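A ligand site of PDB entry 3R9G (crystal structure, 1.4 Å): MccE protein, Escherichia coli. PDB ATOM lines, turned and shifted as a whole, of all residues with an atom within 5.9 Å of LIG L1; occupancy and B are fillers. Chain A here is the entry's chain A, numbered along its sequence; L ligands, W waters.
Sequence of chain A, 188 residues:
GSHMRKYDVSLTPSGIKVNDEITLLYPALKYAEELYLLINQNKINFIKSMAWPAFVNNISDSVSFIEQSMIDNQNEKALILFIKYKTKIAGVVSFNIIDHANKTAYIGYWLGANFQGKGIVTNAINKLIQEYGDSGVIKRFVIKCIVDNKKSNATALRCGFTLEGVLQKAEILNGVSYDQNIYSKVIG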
ATOM      1  N   ASN A  45      17.685 -30.684  37.399  1.00  0.00           N
ATOM      2  CA  ASN A  45      17.541 -29.387  36.745  1.00  0.00           C
ATOM      3  C   ASN A  45      16.911 -29.483  35.341  1.00  0.00           C
ATOM      4  O   ASN A  45      16.094 -28.634  34.974  1.00  0.00           O
ATOM      5  CB  ASN A  45      18.850 -28.562  36.723  1.00  0.00           C
ATOM      6  CG  ASN A  45      20.099 -29.396  36.378  1.00  0.00           C
ATOM      7  OD1 ASN A  45      20.444 -30.354  37.070  1.00  0.00           O
ATOM      8  ND2 ASN A  45      20.817 -28.976  35.324  1.00  0.00           N
ATOM      9  N   PHE A  46      17.273 -30.519  34.598  1.00  0.00           N
ATOM     10  CA  PHE A  46      16.780 -30.668  33.218  1.00  0.00           C
ATOM     11  C   PHE A  46      15.288 -30.940  33.123  1.00  0.00           C
ATOM     12  O   PHE A  46      14.636 -30.526  32.160  1.00  0.00           O
ATOM     13  CB  PHE A  46      17.523 -31.789  32.472  1.00  0.00           C
ATOM     14  CG  PHE A  46      18.895 -31.411  31.990  1.00  0.00           C
ATOM     15  CD1 PHE A  46      19.432 -30.138  32.185  1.00  0.00           C
ATOM     16  CD2 PHE A  46      19.645 -32.348  31.289  1.00  0.00           C
ATOM     17  CE1 PHE A  46      20.691 -29.814  31.711  1.00  0.00           C
ATOM     18  CE2 PHE A  46      20.901 -32.032  30.810  1.00  0.00           C
ATOM     19  CZ  PHE A  46      21.430 -30.762  31.033  1.00  0.00           C
ATOM     20  N   SER A  49      12.857 -28.101  32.280  1.00  0.00           N
ATOM     21  CA  SER A  49      12.821 -27.451  30.967  1.00  0.00           C
ATOM     22  C   SER A  49      12.607 -28.393  29.780  1.00  0.00           C
ATOM     23  O   SER A  49      12.368 -27.926  28.668  1.00  0.00           O
ATOM     24  CB  SER A  49      14.094 -26.632  30.747  1.00  0.00           C
ATOM     25  OG  SER A  49      15.224 -27.470  30.790  1.00  0.00           O
ATOM     26  N   MET A  50      12.697 -29.698  30.006  1.00  0.00           N
ATOM     27  CA  MET A  50      12.569 -30.697  28.947  1.00  0.00           C
ATOM     28  C   MET A  50      11.823 -31.930  29.453  1.00  0.00           C
ATOM     29  O   MET A  50      11.835 -32.205  30.655  1.00  0.00           O
ATOM     30  CB  MET A  50      13.965 -31.097  28.416  1.00  0.00           C
ATOM     31  CG  MET A  50      14.780 -29.928  27.857  1.00  0.00           C
ATOM     32  SD  MET A  50      16.414 -30.380  27.235  1.00  0.00           S
ATOM     33  CE  MET A  50      17.242 -30.833  28.765  1.00  0.00           C
ATOM     34  N   TYR A 109      18.613 -27.589  21.875  1.00  0.00           N
ATOM     35  CA  TYR A 109      19.899 -27.600  22.580  1.00  0.00           C
ATOM     36  C   TYR A 109      19.774 -27.836  24.064  1.00  0.00           C
ATOM     37  O   TYR A 109      18.746 -27.525  24.660  1.00  0.00           O
ATOM     38  CB  TYR A 109      20.678 -26.287  22.348  1.00  0.00           C
ATOM     39  CG  TYR A 109      19.856 -25.011  22.398  1.00  0.00           C
ATOM     40  CD1 TYR A 109      19.424 -24.460  23.606  1.00  0.00           C
ATOM     41  CD2 TYR A 109      19.528 -24.346  21.218  1.00  0.00           C
ATOM     42  CE1 TYR A 109      18.685 -23.278  23.628  1.00  0.00           C
ATOM     43  CE2 TYR A 109      18.795 -23.172  21.231  1.00  0.00           C
ATOM     44  CZ  TYR A 109      18.375 -22.634  22.438  1.00  0.00           C
ATOM     45  OH  TYR A 109      17.650 -21.468  22.440  1.00  0.00           O
ATOM     46  N   TRP A 110      20.845 -28.370  24.649  1.00  0.00           N
ATOM     47  CA  TRP A 110      21.029 -28.366  26.101  1.00  0.00           C
ATOM     48  C   TRP A 110      22.512 -28.456  26.453  1.00  0.00           C
ATOM     49  O   TRP A 110      23.309 -28.983  25.680  1.00  0.00           O
ATOM     50  CB  TRP A 110      20.250 -29.490  26.792  1.00  0.00           C
ATOM     51  CG  TRP A 110      20.643 -30.906  26.484  1.00  0.00           C
ATOM     52  CD1 TRP A 110      20.007 -31.753  25.618  1.00  0.00           C
ATOM     53  CD2 TRP A 110      21.672 -31.690  27.130  1.00  0.00           C
ATOM     54  NE1 TRP A 110      20.601 -32.998  25.654  1.00  0.00           N
ATOM     55  CE2 TRP A 110      21.624 -32.981  26.580  1.00  0.00           C
ATOM     56  CE3 TRP A 110      22.652 -31.408  28.101  1.00  0.00           C
ATOM     57  CZ2 TRP A 110      22.505 -34.006  26.963  1.00  0.00           C
ATOM     58  CZ3 TRP A 110      23.522 -32.420  28.487  1.00  0.00           C
ATOM     59  CH2 TRP A 110      23.433 -33.706  27.921  1.00  0.00           C
ATOM     60  N   LEU A 111      22.839 -27.953  27.648  1.00  0.00           N
ATOM     61  CA  LEU A 111      24.174 -28.052  28.227  1.00  0.00           C
ATOM     62  C   LEU A 111      24.091 -28.500  29.675  1.00  0.00           C
ATOM     63  O   LEU A 111      23.215 -28.051  30.407  1.00  0.00           O
ATOM     64  CB  LEU A 111      24.865 -26.690  28.220  1.00  0.00           C
ATOM     65  CG  LEU A 111      25.305 -26.114  26.875  1.00  0.00           C
ATOM     66  CD1 LEU A 111      25.731 -24.679  27.094  1.00  0.00           C
ATOM     67  CD2 LEU A 111      26.428 -26.939  26.258  1.00  0.00           C
ATOM     68  N   GLY A 112      25.028 -29.350  30.085  1.00  0.00           N
ATOM     69  CA  GLY A 112      25.168 -29.642  31.513  1.00  0.00           C
ATOM     70  C   GLY A 112      25.458 -28.360  32.276  1.00  0.00           C
ATOM     71  O   GLY A 112      26.050 -27.422  31.723  1.00  0.00           O
ATOM     72  N   PHE A 115      28.758 -26.564  32.154  1.00  0.00           N
ATOM     73  CA  PHE A 115      29.142 -26.057  30.844  1.00  0.00           C
ATOM     74  C   PHE A 115      28.379 -24.798  30.442  1.00  0.00           C
ATOM     75  O   PHE A 115      28.640 -24.212  29.381  1.00  0.00           O
ATOM     76  CB  PHE A 115      28.980 -27.147  29.791  1.00  0.00           C
ATOM     77  CG  PHE A 115      29.801 -28.363  30.061  1.00  0.00           C
ATOM     78  CD1 PHE A 115      31.146 -28.391  29.695  1.00  0.00           C
ATOM     79  CD2 PHE A 115      29.247 -29.462  30.694  1.00  0.00           C
ATOM     80  CE1 PHE A 115      31.934 -29.512  29.955  1.00  0.00           C
ATOM     81  CE2 PHE A 115      30.017 -30.607  30.960  1.00  0.00           C
ATOM     82  CZ  PHE A 115      31.369 -30.620  30.587  1.00  0.00           C
ATOM     83  N   GLN A 116      27.450 -24.386  31.295  1.00  0.00           N
ATOM     84  CA  GLN A 116      26.664 -23.181  31.053  1.00  0.00           C
ATOM     85  C   GLN A 116      27.461 -21.942  31.420  1.00  0.00           C
ATOM     86  O   GLN A 116      28.379 -22.003  32.253  1.00  0.00           O
ATOM     87  CB  GLN A 116      25.343 -23.250  31.814  1.00  0.00           C
ATOM     88  CG  GLN A 116      24.417 -24.343  31.283  1.00  0.00           C
ATOM     89  CD  GLN A 116      23.163 -24.529  32.101  1.00  0.00           C
ATOM     90  OE1 GLN A 116      22.744 -23.634  32.842  1.00  0.00           O
ATOM     91  NE2 GLN A 116      22.549 -25.686  31.973  1.00  0.00           N
ATOM     92  N   GLY A 117      27.130 -20.810  30.789  1.00  0.00           N
ATOM     93  CA  GLY A 117      27.813 -19.550  31.058  1.00  0.00           C
ATOM     94  C   GLY A 117      29.113 -19.369  30.293  1.00  0.00           C
ATOM     95  O   GLY A 117      29.903 -18.493  30.638  1.00  0.00           O
ATOM     96  N   LYS A 118      29.299 -20.158  29.231  1.00  0.00           N
ATOM     97  CA  LYS A 118      30.542 -20.173  28.478  1.00  0.00           C
ATOM     98  C   LYS A 118      30.353 -19.863  26.995  1.00  0.00           C
ATOM     99  O   LYS A 118      31.289 -19.962  26.209  1.00  0.00           O
ATOM    100  CB  LYS A 118      31.226 -21.544  28.618  1.00  0.00           C
ATOM    101  CG  LYS A 118      31.748 -21.877  30.006  1.00  0.00           C
ATOM    102  CD  LYS A 118      32.279 -23.300  30.045  1.00  0.00           C
ATOM    103  CE  LYS A 118      32.965 -23.642  31.356  1.00  0.00           C
ATOM    104  NZ  LYS A 118      34.293 -22.993  31.466  1.00  0.00           N
ATOM    105  N   GLY A 119      29.146 -19.472  26.618  1.00  0.00           N
ATOM    106  CA  GLY A 119      28.829 -19.182  25.213  1.00  0.00           C
ATOM    107  C   GLY A 119      28.861 -20.380  24.277  1.00  0.00           C
ATOM    108  O   GLY A 119      28.915 -20.214  23.058  1.00  0.00           O
ATOM    109  N   ILE A 120      28.816 -21.588  24.825  1.00  0.00           N
ATOM    110  CA  ILE A 120      29.012 -22.781  24.006  1.00  0.00           C
ATOM    111  C   ILE A 120      27.892 -22.993  22.983  1.00  0.00           C
ATOM    112  O   ILE A 120      28.163 -23.283  21.825  1.00  0.00           O
ATOM    113  CB  ILE A 120      29.197 -24.037  24.877  1.00  0.00           C
ATOM    114  CG1 ILE A 120      30.537 -23.960  25.615  1.00  0.00           C
ATOM    115  CG2 ILE A 120      29.125 -25.329  24.035  1.00  0.00           C
ATOM    116  CD1 ILE A 120      30.659 -24.939  26.776  1.00  0.00           C
ATOM    117  N   VAL A 121      26.630 -22.839  23.406  1.00  0.00           N
ATOM    118  CA  VAL A 121      25.524 -23.052  22.481  1.00  0.00           C
ATOM    119  C   VAL A 121      25.415 -21.896  21.475  1.00  0.00           C
ATOM    120  O   VAL A 121      25.186 -22.133  20.294  1.00  0.00           O
ATOM    121  CB  VAL A 121      24.200 -23.313  23.230  1.00  0.00           C
ATOM    122  CG1 VAL A 121      22.993 -23.116  22.322  1.00  0.00           C
ATOM    123  CG2 VAL A 121      24.191 -24.727  23.775  1.00  0.00           C
ATOM    124  N   THR A 122      25.619 -20.658  21.922  1.00  0.00           N
ATOM    125  CA  THR A 122      25.642 -19.542  20.979  1.00  0.00           C
ATOM    126  C   THR A 122      26.701 -19.759  19.891  1.00  0.00           C
ATOM    127  O   THR A 122      26.416 -19.591  18.702  1.00  0.00           O
ATOM    128  CB  THR A 122      25.858 -18.190  21.710  1.00  0.00           C
ATOM    129  OG1 THR A 122      24.650 -17.862  22.398  1.00  0.00           O
ATOM    130  CG2 THR A 122      26.173 -17.064  20.730  1.00  0.00           C
ATOM    131  N   ASN A 123      27.913 -20.177  20.273  1.00  0.00           N
ATOM    132  CA  ASN A 123      28.953 -20.445  19.279  1.00  0.00           C
ATOM    133  C   ASN A 123      28.563 -21.586  18.348  1.00  0.00           C
ATOM    134  O   ASN A 123      28.786 -21.521  17.144  1.00  0.00           O
ATOM    135  CB  ASN A 123      30.284 -20.767  19.957  1.00  0.00           C
ATOM    136  CG  ASN A 123      31.007 -19.553  20.451  1.00  0.00           C
ATOM    137  OD1 ASN A 123      31.053 -18.520  19.782  1.00  0.00           O
ATOM    138  ND2 ASN A 123      31.653 -19.682  21.613  1.00  0.00           N
ATOM    139  N   LYS A 144      12.110 -22.509  19.075  1.00  0.00           N
ATOM    140  CA  LYS A 144      10.922 -22.434  19.907  1.00  0.00           C
ATOM    141  C   LYS A 144      11.315 -22.706  21.337  1.00  0.00           C
ATOM    142  O   LYS A 144      11.992 -23.688  21.618  1.00  0.00           O
ATOM    143  CB  LYS A 144       9.883 -23.471  19.499  1.00  0.00           C
ATOM    144  CG  LYS A 144       9.415 -23.385  18.071  1.00  0.00           C
ATOM    145  CD  LYS A 144       8.425 -24.501  17.781  1.00  0.00           C
ATOM    146  CE  LYS A 144       7.869 -24.433  16.372  1.00  0.00           C
ATOM    147  NZ  LYS A 144       6.876 -25.527  16.126  1.00  0.00           N
ATOM    148  N   CYS A 145      10.863 -21.855  22.263  1.00  0.00           N
ATOM    149  CA  CYS A 145      11.164 -22.104  23.664  1.00  0.00           C
ATOM    150  C   CYS A 145      10.107 -21.537  24.597  1.00  0.00           C
ATOM    151  O   CYS A 145       9.540 -20.480  24.352  1.00  0.00           O
ATOM    152  CB  CYS A 145      12.555 -21.585  24.035  1.00  0.00           C
ATOM    153  SG  CYS A 145      12.817 -19.851  23.660  1.00  0.00           S
ATOM    154  N   ILE A 146       9.862 -22.263  25.672  1.00  0.00           N
ATOM    155  CA  ILE A 146       8.866 -21.870  26.639  1.00  0.00           C
ATOM    156  C   ILE A 146       9.142 -20.434  27.107  1.00  0.00           C
ATOM    157  O   ILE A 146      10.290 -20.054  27.334  1.00  0.00           O
ATOM    158  CB  ILE A 146       8.783 -22.900  27.777  1.00  0.00           C
ATOM    159  CG1 ILE A 146       8.019 -24.131  27.266  1.00  0.00           C
ATOM    160  CG2 ILE A 146       8.114 -22.336  29.024  1.00  0.00           C
ATOM    161  CD1 ILE A 146       8.098 -25.351  28.150  1.00  0.00           C
ATOM    162  N   ASN A 149      11.410 -19.768  30.070  1.00  0.00           N
ATOM    163  CA  ASN A 149      12.755 -20.328  30.049  1.00  0.00           C
ATOM    164  C   ASN A 149      13.744 -19.203  29.765  1.00  0.00           C
ATOM    165  O   ASN A 149      14.063 -18.917  28.612  1.00  0.00           O
ATOM    166  CB  ASN A 149      12.883 -21.455  29.021  1.00  0.00           C
ATOM    167  CG  ASN A 149      14.199 -22.198  29.100  1.00  0.00           C
ATOM    168  OD1 ASN A 149      15.247 -21.635  29.452  1.00  0.00           O
ATOM    169  ND2 ASN A 149      14.175 -23.469  28.748  1.00  0.00           N
ATOM    170  N   LYS A 151      17.039 -18.595  30.184  1.00  0.00           N
ATOM    171  CA  LYS A 151      18.308 -18.811  29.503  1.00  0.00           C
ATOM    172  C   LYS A 151      18.138 -19.167  28.026  1.00  0.00           C
ATOM    173  O   LYS A 151      18.919 -18.719  27.183  1.00  0.00           O
ATOM    174  CB  LYS A 151      19.166 -19.858  30.213  1.00  0.00           C
ATOM    175  CG  LYS A 151      19.581 -19.467  31.629  1.00  0.00           C
ATOM    176  CD  LYS A 151      20.527 -18.266  31.670  1.00  0.00           C
ATOM    177  CE  LYS A 151      21.083 -18.051  33.076  1.00  0.00           C
ATOM    178  NZ  LYS A 151      21.893 -19.217  33.544  1.00  0.00           N
ATOM    179  N   SER A 152      17.104 -19.934  27.696  1.00  0.00           N
ATOM    180  CA  SER A 152      16.914 -20.316  26.290  1.00  0.00           C
ATOM    181  C   SER A 152      16.496 -19.117  25.433  1.00  0.00           C
ATOM    182  O   SER A 152      16.995 -18.947  24.318  1.00  0.00           O
ATOM    183  CB  SER A 152      15.939 -21.473  26.123  1.00  0.00           C
ATOM    184  OG  SER A 152      15.895 -21.833  24.750  1.00  0.00           O
ATOM    185  N   ALA A 154      17.278 -16.023  26.114  1.00  0.00           N
ATOM    186  CA  ALA A 154      18.474 -15.198  25.991  1.00  0.00           C
ATOM    187  C   ALA A 154      19.416 -15.713  24.889  1.00  0.00           C
ATOM    188  O   ALA A 154      19.965 -14.924  24.124  1.00  0.00           O
ATOM    189  CB  ALA A 154      19.193 -15.102  27.324  1.00  0.00           C
ATOM    190  N   THR A 155      19.559 -17.040  24.796  1.00  0.00           N
ATOM    191  CA  THR A 155      20.367 -17.654  23.747  1.00  0.00           C
ATOM    192  C   THR A 155      19.836 -17.320  22.338  1.00  0.00           C
ATOM    193  O   THR A 155      20.592 -16.927  21.456  1.00  0.00           O
ATOM    194  CB  THR A 155      20.502 -19.176  23.986  1.00  0.00           C
ATOM    195  OG1 THR A 155      21.252 -19.389  25.195  1.00  0.00           O
ATOM    196  CG2 THR A 155      21.221 -19.861  22.828  1.00  0.00           C
ATOM    197  N   ARG A 158      20.710 -13.763  21.642  1.00  0.00           N
ATOM    198  CA  ARG A 158      22.172 -13.644  21.528  1.00  0.00           C
ATOM    199  C   ARG A 158      22.668 -14.103  20.140  1.00  0.00           C
ATOM    200  O   ARG A 158      23.674 -13.611  19.647  1.00  0.00           O
ATOM    201  CB  ARG A 158      22.841 -14.473  22.631  1.00  0.00           C
ATOM    202  CG  ARG A 158      24.331 -14.262  22.831  1.00  0.00           C
ATOM    203  CD  ARG A 158      24.801 -15.033  24.062  1.00  0.00           C
ATOM    204  NE  ARG A 158      24.287 -14.466  25.310  1.00  0.00           N
ATOM    205  CZ  ARG A 158      23.366 -15.027  26.094  1.00  0.00           C
ATOM    206  NH1 ARG A 158      22.818 -16.216  25.818  1.00  0.00           N
ATOM    207  NH2 ARG A 158      22.986 -14.398  27.212  1.00  0.00           N
ATOM    208  N   GLU A 171       3.810 -26.438  24.283  1.00  0.00           N
ATOM    209  CA  GLU A 171       4.770 -27.423  24.772  1.00  0.00           C
ATOM    210  C   GLU A 171       4.312 -27.997  26.101  1.00  0.00           C
ATOM    211  O   GLU A 171       4.048 -27.259  27.036  1.00  0.00           O
ATOM    212  CB  GLU A 171       6.169 -26.816  24.910  1.00  0.00           C
ATOM    213  CG  GLU A 171       7.244 -27.882  25.179  1.00  0.00           C
ATOM    214  CD  GLU A 171       8.659 -27.357  25.172  1.00  0.00           C
ATOM    215  OE1 GLU A 171       8.891 -26.196  24.760  1.00  0.00           O
ATOM    216  OE2 GLU A 171       9.544 -28.137  25.578  1.00  0.00           O
HETATM  217  N1  LIG L   1      30.056 -15.994  23.884  1.00  0.00           N
HETATM  218  C1  LIG L   1      28.905 -15.737  24.374  1.00  0.00           C
HETATM  219  N2  LIG L   1      28.590 -15.891  25.603  1.00  0.00           N
HETATM  220  C2  LIG L   1      29.576 -16.180  26.521  1.00  0.00           C
HETATM  221  C3  LIG L   1      30.841 -16.392  26.095  1.00  0.00           C
HETATM  222  C4  LIG L   1      31.091 -16.360  24.657  1.00  0.00           C
HETATM  223  N3  LIG L   1      32.241 -16.825  24.181  1.00  0.00           N
HETATM  224  N4  LIG L   1      31.584 -16.673  27.182  1.00  0.00           N
HETATM  225  C5  LIG L   1      30.743 -16.579  28.245  1.00  0.00           C
HETATM  226  N5  LIG L   1      29.495 -16.258  27.840  1.00  0.00           N
HETATM  227  C6  LIG L   1      28.321 -16.218  28.747  1.00  0.00           C
HETATM  228  C7  LIG L   1      27.259 -15.172  28.549  1.00  0.00           C
HETATM  229  O1  LIG L   1      27.537 -14.019  29.335  1.00  0.00           O
HETATM  230  C8  LIG L   1      26.016 -15.899  29.041  1.00  0.00           C
HETATM  231  O2  LIG L   1      26.057 -16.031  30.471  1.00  0.00           O
HETATM  232  P1  LIG L   1      24.913 -15.421  31.439  1.00  0.00           P
HETATM  233  O3  LIG L   1      25.554 -15.411  32.806  1.00  0.00           O
HETATM  234  O4  LIG L   1      23.714 -16.316  31.304  1.00  0.00           O
HETATM  235  O5  LIG L   1      24.623 -14.049  30.886  1.00  0.00           O
HETATM  236  C9  LIG L   1      26.221 -17.304  28.519  1.00  0.00           C
HETATM  237  O6  LIG L   1      27.649 -17.466  28.454  1.00  0.00           O
HETATM  238  C10 LIG L   1      25.588 -17.519  27.138  1.00  0.00           C
HETATM  239  O7  LIG L   1      25.951 -18.807  26.644  1.00  0.00           O
HETATM  240  P2  LIG L   1      25.024 -19.602  25.607  1.00  0.00           P
HETATM  241  O8  LIG L   1      24.028 -18.662  24.986  1.00  0.00           O
HETATM  242  O9  LIG L   1      25.922 -20.378  24.703  1.00  0.00           O
HETATM  243  O10 LIG L   1      24.219 -20.680  26.489  1.00  0.00           O
HETATM  244  P3  LIG L   1      24.121 -20.883  28.087  1.00  0.00           P
HETATM  245  O11 LIG L   1      25.447 -21.348  28.590  1.00  0.00           O
HETATM  246  O12 LIG L   1      23.501 -19.690  28.727  1.00  0.00           O
HETATM  247  O13 LIG L   1      23.130 -22.126  28.132  1.00  0.00           O
HETATM  248  C11 LIG L   1      20.995 -23.244  27.729  1.00  0.00           C
HETATM  249  C12 LIG L   1      21.757 -21.923  27.749  1.00  0.00           C
HETATM  250  C13 LIG L   1      19.545 -22.941  27.363  1.00  0.00           C
HETATM  251  C14 LIG L   1      21.640 -24.134  26.665  1.00  0.00           C
HETATM  252  C15 LIG L   1      21.121 -23.865  29.122  1.00  0.00           C
HETATM  253  O14 LIG L   1      20.580 -22.956  30.080  1.00  0.00           O
HETATM  254  C16 LIG L   1      20.442 -25.209  29.254  1.00  0.00           C
HETATM  255  O15 LIG L   1      20.952 -26.213  28.788  1.00  0.00           O
HETATM  256  N6  LIG L   1      19.285 -25.252  29.897  1.00  0.00           N
HETATM  257  C17 LIG L   1      18.465 -26.445  30.179  1.00  0.00           C
HETATM  258  C18 LIG L   1      17.973 -27.095  28.888  1.00  0.00           C
HETATM  259  C19 LIG L   1      17.138 -26.132  28.095  1.00  0.00           C
HETATM  260  O16 LIG L   1      16.443 -25.292  28.661  1.00  0.00           O
HETATM  261  N7  LIG L   1      17.204 -26.211  26.767  1.00  0.00           N
HETATM  262  C20 LIG L   1      16.491 -25.376  25.809  1.00  0.00           C
HETATM  263  C21 LIG L   1      15.028 -25.773  25.876  1.00  0.00           C
HETATM  264  S1  LIG L   1      14.068 -24.526  25.001  1.00  0.00           S
HETATM  265  C1  LG2 L   2      13.438 -28.435  22.295  1.00  0.00           C
HETATM  266  N1  LG2 L   2      13.634 -25.986  21.868  1.00  0.00           N
HETATM  267  O1  LG2 L   2      13.999 -28.748  21.237  1.00  0.00           O
HETATM  268  P1  LG2 L   2      13.850 -30.858  23.352  1.00  0.00           P
HETATM  269  N2  LG2 L   2      19.224 -37.686  25.102  1.00  0.00           N
HETATM  270  C2  LG2 L   2      20.012 -36.624  24.851  1.00  0.00           C
HETATM  271  N3  LG2 L   2      19.563 -35.517  24.223  1.00  0.00           N
HETATM  272  C3  LG2 L   2      18.266 -35.478  23.833  1.00  0.00           C
HETATM  273  C4  LG2 L   2      17.415 -36.554  24.067  1.00  0.00           C
HETATM  274  C5  LG2 L   2      17.924 -37.689  24.724  1.00  0.00           C
HETATM  275  N4  LG2 L   2      17.139 -38.757  24.982  1.00  0.00           N
HETATM  276  N5  LG2 L   2      16.206 -36.225  23.556  1.00  0.00           N
HETATM  277  C6  LG2 L   2      16.299 -34.999  23.022  1.00  0.00           C
HETATM  278  N6  LG2 L   2      13.294 -29.223  23.341  1.00  0.00           N
HETATM  279  N7  LG2 L   2      17.562 -34.550  23.174  1.00  0.00           N
HETATM  280  C7  LG2 L   2      12.881 -27.061  22.527  1.00  0.00           C
HETATM  281  C8  LG2 L   2      11.369 -26.945  22.260  1.00  0.00           C
HETATM  282  C9  LG2 L   2      10.847 -27.336  20.900  1.00  0.00           C
HETATM  283  C10 LG2 L   2      18.104 -33.248  22.739  1.00  0.00           C
HETATM  284  O2  LG2 L   2      13.787 -31.404  24.801  1.00  0.00           O
HETATM  285  C11 LG2 L   2      17.610 -32.788  21.384  1.00  0.00           C
HETATM  286  O3  LG2 L   2      18.360 -33.398  20.329  1.00  0.00           O
HETATM  287  C12 LG2 L   2      17.798 -31.279  21.459  1.00  0.00           C
HETATM  288  O4  LG2 L   2      19.105 -30.854  21.057  1.00  0.00           O
HETATM  289  O5  LG2 L   2      12.960 -31.734  22.359  1.00  0.00           O
HETATM  290  C13 LG2 L   2      13.228 -31.892  20.978  1.00  0.00           C
HETATM  291  C14 LG2 L   2      11.983 -32.481  20.339  1.00  0.00           C
HETATM  292  C15 LG2 L   2      10.913 -31.406  20.153  1.00  0.00           C
HETATM  293  N8  LG2 L   2       9.605 -32.031  20.115  1.00  0.00           N
HETATM  294  C16 LG2 L   2      14.969 -25.820  22.036  1.00  0.00           C
HETATM  295  C17 LG2 L   2      15.644 -26.717  22.733  1.00  0.00           C
HETATM  296  O6  LG2 L   2      15.600 -24.876  21.521  1.00  0.00           O
HETATM  297  C18 LG2 L   2      17.678 -30.976  22.944  1.00  0.00           C
HETATM  298  O7  LG2 L   2      17.623 -32.237  23.604  1.00  0.00           O
HETATM  299  C19 LG2 L   2      16.407 -30.219  23.326  1.00  0.00           C
HETATM  300  O8  LG2 L   2      15.314 -30.914  22.734  1.00  0.00           O
HETATM  301  O9  LG2 L   2       9.676 -27.803  20.848  1.00  0.00           O
HETATM  302  O10 LG2 L   2      11.534 -27.155  19.882  1.00  0.00           O
HETATM  303  O   HOH W   1      21.591 -17.966  27.903  1.00  0.00           O
HETATM  304  O   HOH W   2      11.009 -24.865  25.806  1.00  0.00           O
HETATM  305  O   HOH W   3      34.227 -18.491  22.263  1.00  0.00           O
HETATM  306  O   HOH W   4      27.926 -22.130  27.663  1.00  0.00           O
HETATM  307  O   HOH W   5      17.110 -23.279  30.857  1.00  0.00           O
HETATM  308  O   HOH W   6      24.198 -19.028  31.227  1.00  0.00           O
HETATM  309  O   HOH W   7      16.604 -26.857  33.064  1.00  0.00           O
HETATM  310  O   HOH W   8      21.788 -15.819  29.508  1.00  0.00           O
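CE of Met 50 touches C18 of LIG L1, at 3.8 Å.
CA of Trp 110 touches O15 of LIG L1, at 3.4 Å.
CA of Gln 116 touches O11 of LIG L1 (3.3 Å).
Asn 123 touches LIG L1 (ND2 to N3, 3.9 Å).
Cys 145 touches LIG L1.
CB of Lys 151 touches O14 of LIG L1, 3.4 Å away.
Hydrophobic or aromatic side chains within 4 Å of LIG L1: Met 50, Tyr 109, Trp 110, Leu 111 and Val 121.
Within 4 Å of LIG L1: Ser 49, Met 50, Tyr 109, Trp 110, Leu 111, Gln 116, Gly 117, Lys 118, Gly 119, Ile 120, Val 121, Thr 122, Asn 123, Cys 145, Asn 149, Lys 151, Ser 152, Thr 155 and Arg 158.
A sulfur (S1) of LIG L1 sits close to a nitrogen (N1) of LG2 L2 (3.5 Å).
NE2 of Gln 116 sits at hydrogen-bond distance from O of Leu 111 (2.9 Å).
The side-chain hydroxyl of Thr 155 sits at hydrogen-bond distance from the backbone carbonyl oxygen of Lys 151 (3.1 Å).
The side-chain amide oxygen of Asn 149 is in hydrogen-bond range of the backbone NH of Ser 152 (3.1 Å).
OH of Tyr 109 sits at hydrogen-bond distance from OG of Ser 152 (2.9 Å).
The backbone carbonyl oxygen of Gly 119 sits at hydrogen-bond distance from the side-chain amide nitrogen of Asn 123, 3.1 Å away.
The side-chain hydroxyl (OG) of Ser 49 is in hydrogen-bond range of the backbone carbonyl oxygen (O) of Phe 46 (3.4 Å).
N of Thr 122 sits at hydrogen-bond distance from O9 of LIG L1 (2.8 Å).
The side-chain hydroxyl (OG1) of Thr 122 lies within hydrogen-bond range of an oxygen (O8) of LIG L1.
An oxygen (O15) of LIG L1 is in hydrogen-bond range of the backbone NH (N) of Leu 111, 2.8 Å away.
The backbone NH (N) of Gly 117 lies within hydrogen-bond range of an oxygen (O11) of LIG L1 (2.8 Å).
The guanidinium group (NH1) of Arg 158 is in salt-bridge range of an oxygen (O8) of LIG L1 (2.9 Å).
An oxygen (O9) of LIG L1 is in hydrogen-bond range of the backbone NH (N) of Val 121 (2.9 Å).
An oxygen (O8) of LIG L1 lies within hydrogen-bond range of the side-chain hydroxyl (OG1) of Thr 155, 2.9 Å away.
O16 of LIG L1 sits at hydrogen-bond distance from ND2 of Asn 149 (2.9 Å).
The backbone carbonyl oxygen (O) of Tyr 109 sits at hydrogen-bond distance from a nitrogen (N7) of LIG L1 (2.9 Å).
N of Gly 119 sits at hydrogen-bond distance from O6 of LIG L1 (3.1 Å).
The backbone NH (N) of Ile 120 sits at hydrogen-bond distance from an oxygen (O9) of LIG L1, 3.1 Å away.
The backbone NH of Lys 118 is in hydrogen-bond range of an oxygen (O6) of LIG L1 (3.3 Å).
OG of Ser 152 lies close to S1 of LIG L1 (3.3 Å).
OG of Ser 49 sits at hydrogen-bond distance from O16 of LIG L1, at 3.3 Å.
The backbone NH (N) of Tyr 109 lies close to an oxygen (O4) of LG2 L2, 3.4 Å away.
N3 of LG2 L2 lies within hydrogen-bond range of NE1 of Trp 110 (3.1 Å).
A nitrogen (N1) of LG2 L2 is in hydrogen-bond range of the backbone carbonyl oxygen of Lys 144 (2.8 Å).
Water W8 lies within hydrogen-bond range of O4 of LIG L1 and NH2 of Arg 158.
Water W1 lies within hydrogen-bond range of O12 of LIG L1 (2.7 Å), O of Lys 151 (2.9 Å), NH1 of Arg 158 (3.0 Å) and OG1 of Thr 155 (3.1 Å).
Water W5 lies within hydrogen-bond range of the side-chain amide oxygen (OD1) of Asn 149 (2.9 Å) and an oxygen (O16) of LIG L1 (3.1 Å).
Water W2 lies within hydrogen-bond range of the side-chain carboxylate (OE1) of Glu 171, the backbone NH (N) of Ile 146 and a sulfur (S1) of LIG L1.
Water W3 bridges the side-chain amide nitrogen (ND2) of Asn 123 (2.9 Å) and a nitrogen (N3) of LIG L1 (3.2 Å).
Water W7 lies within hydrogen-bond range of the backbone carbonyl oxygen of Asn 45 (2.7 Å) and the side-chain hydroxyl of Ser 49 (2.7 Å).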
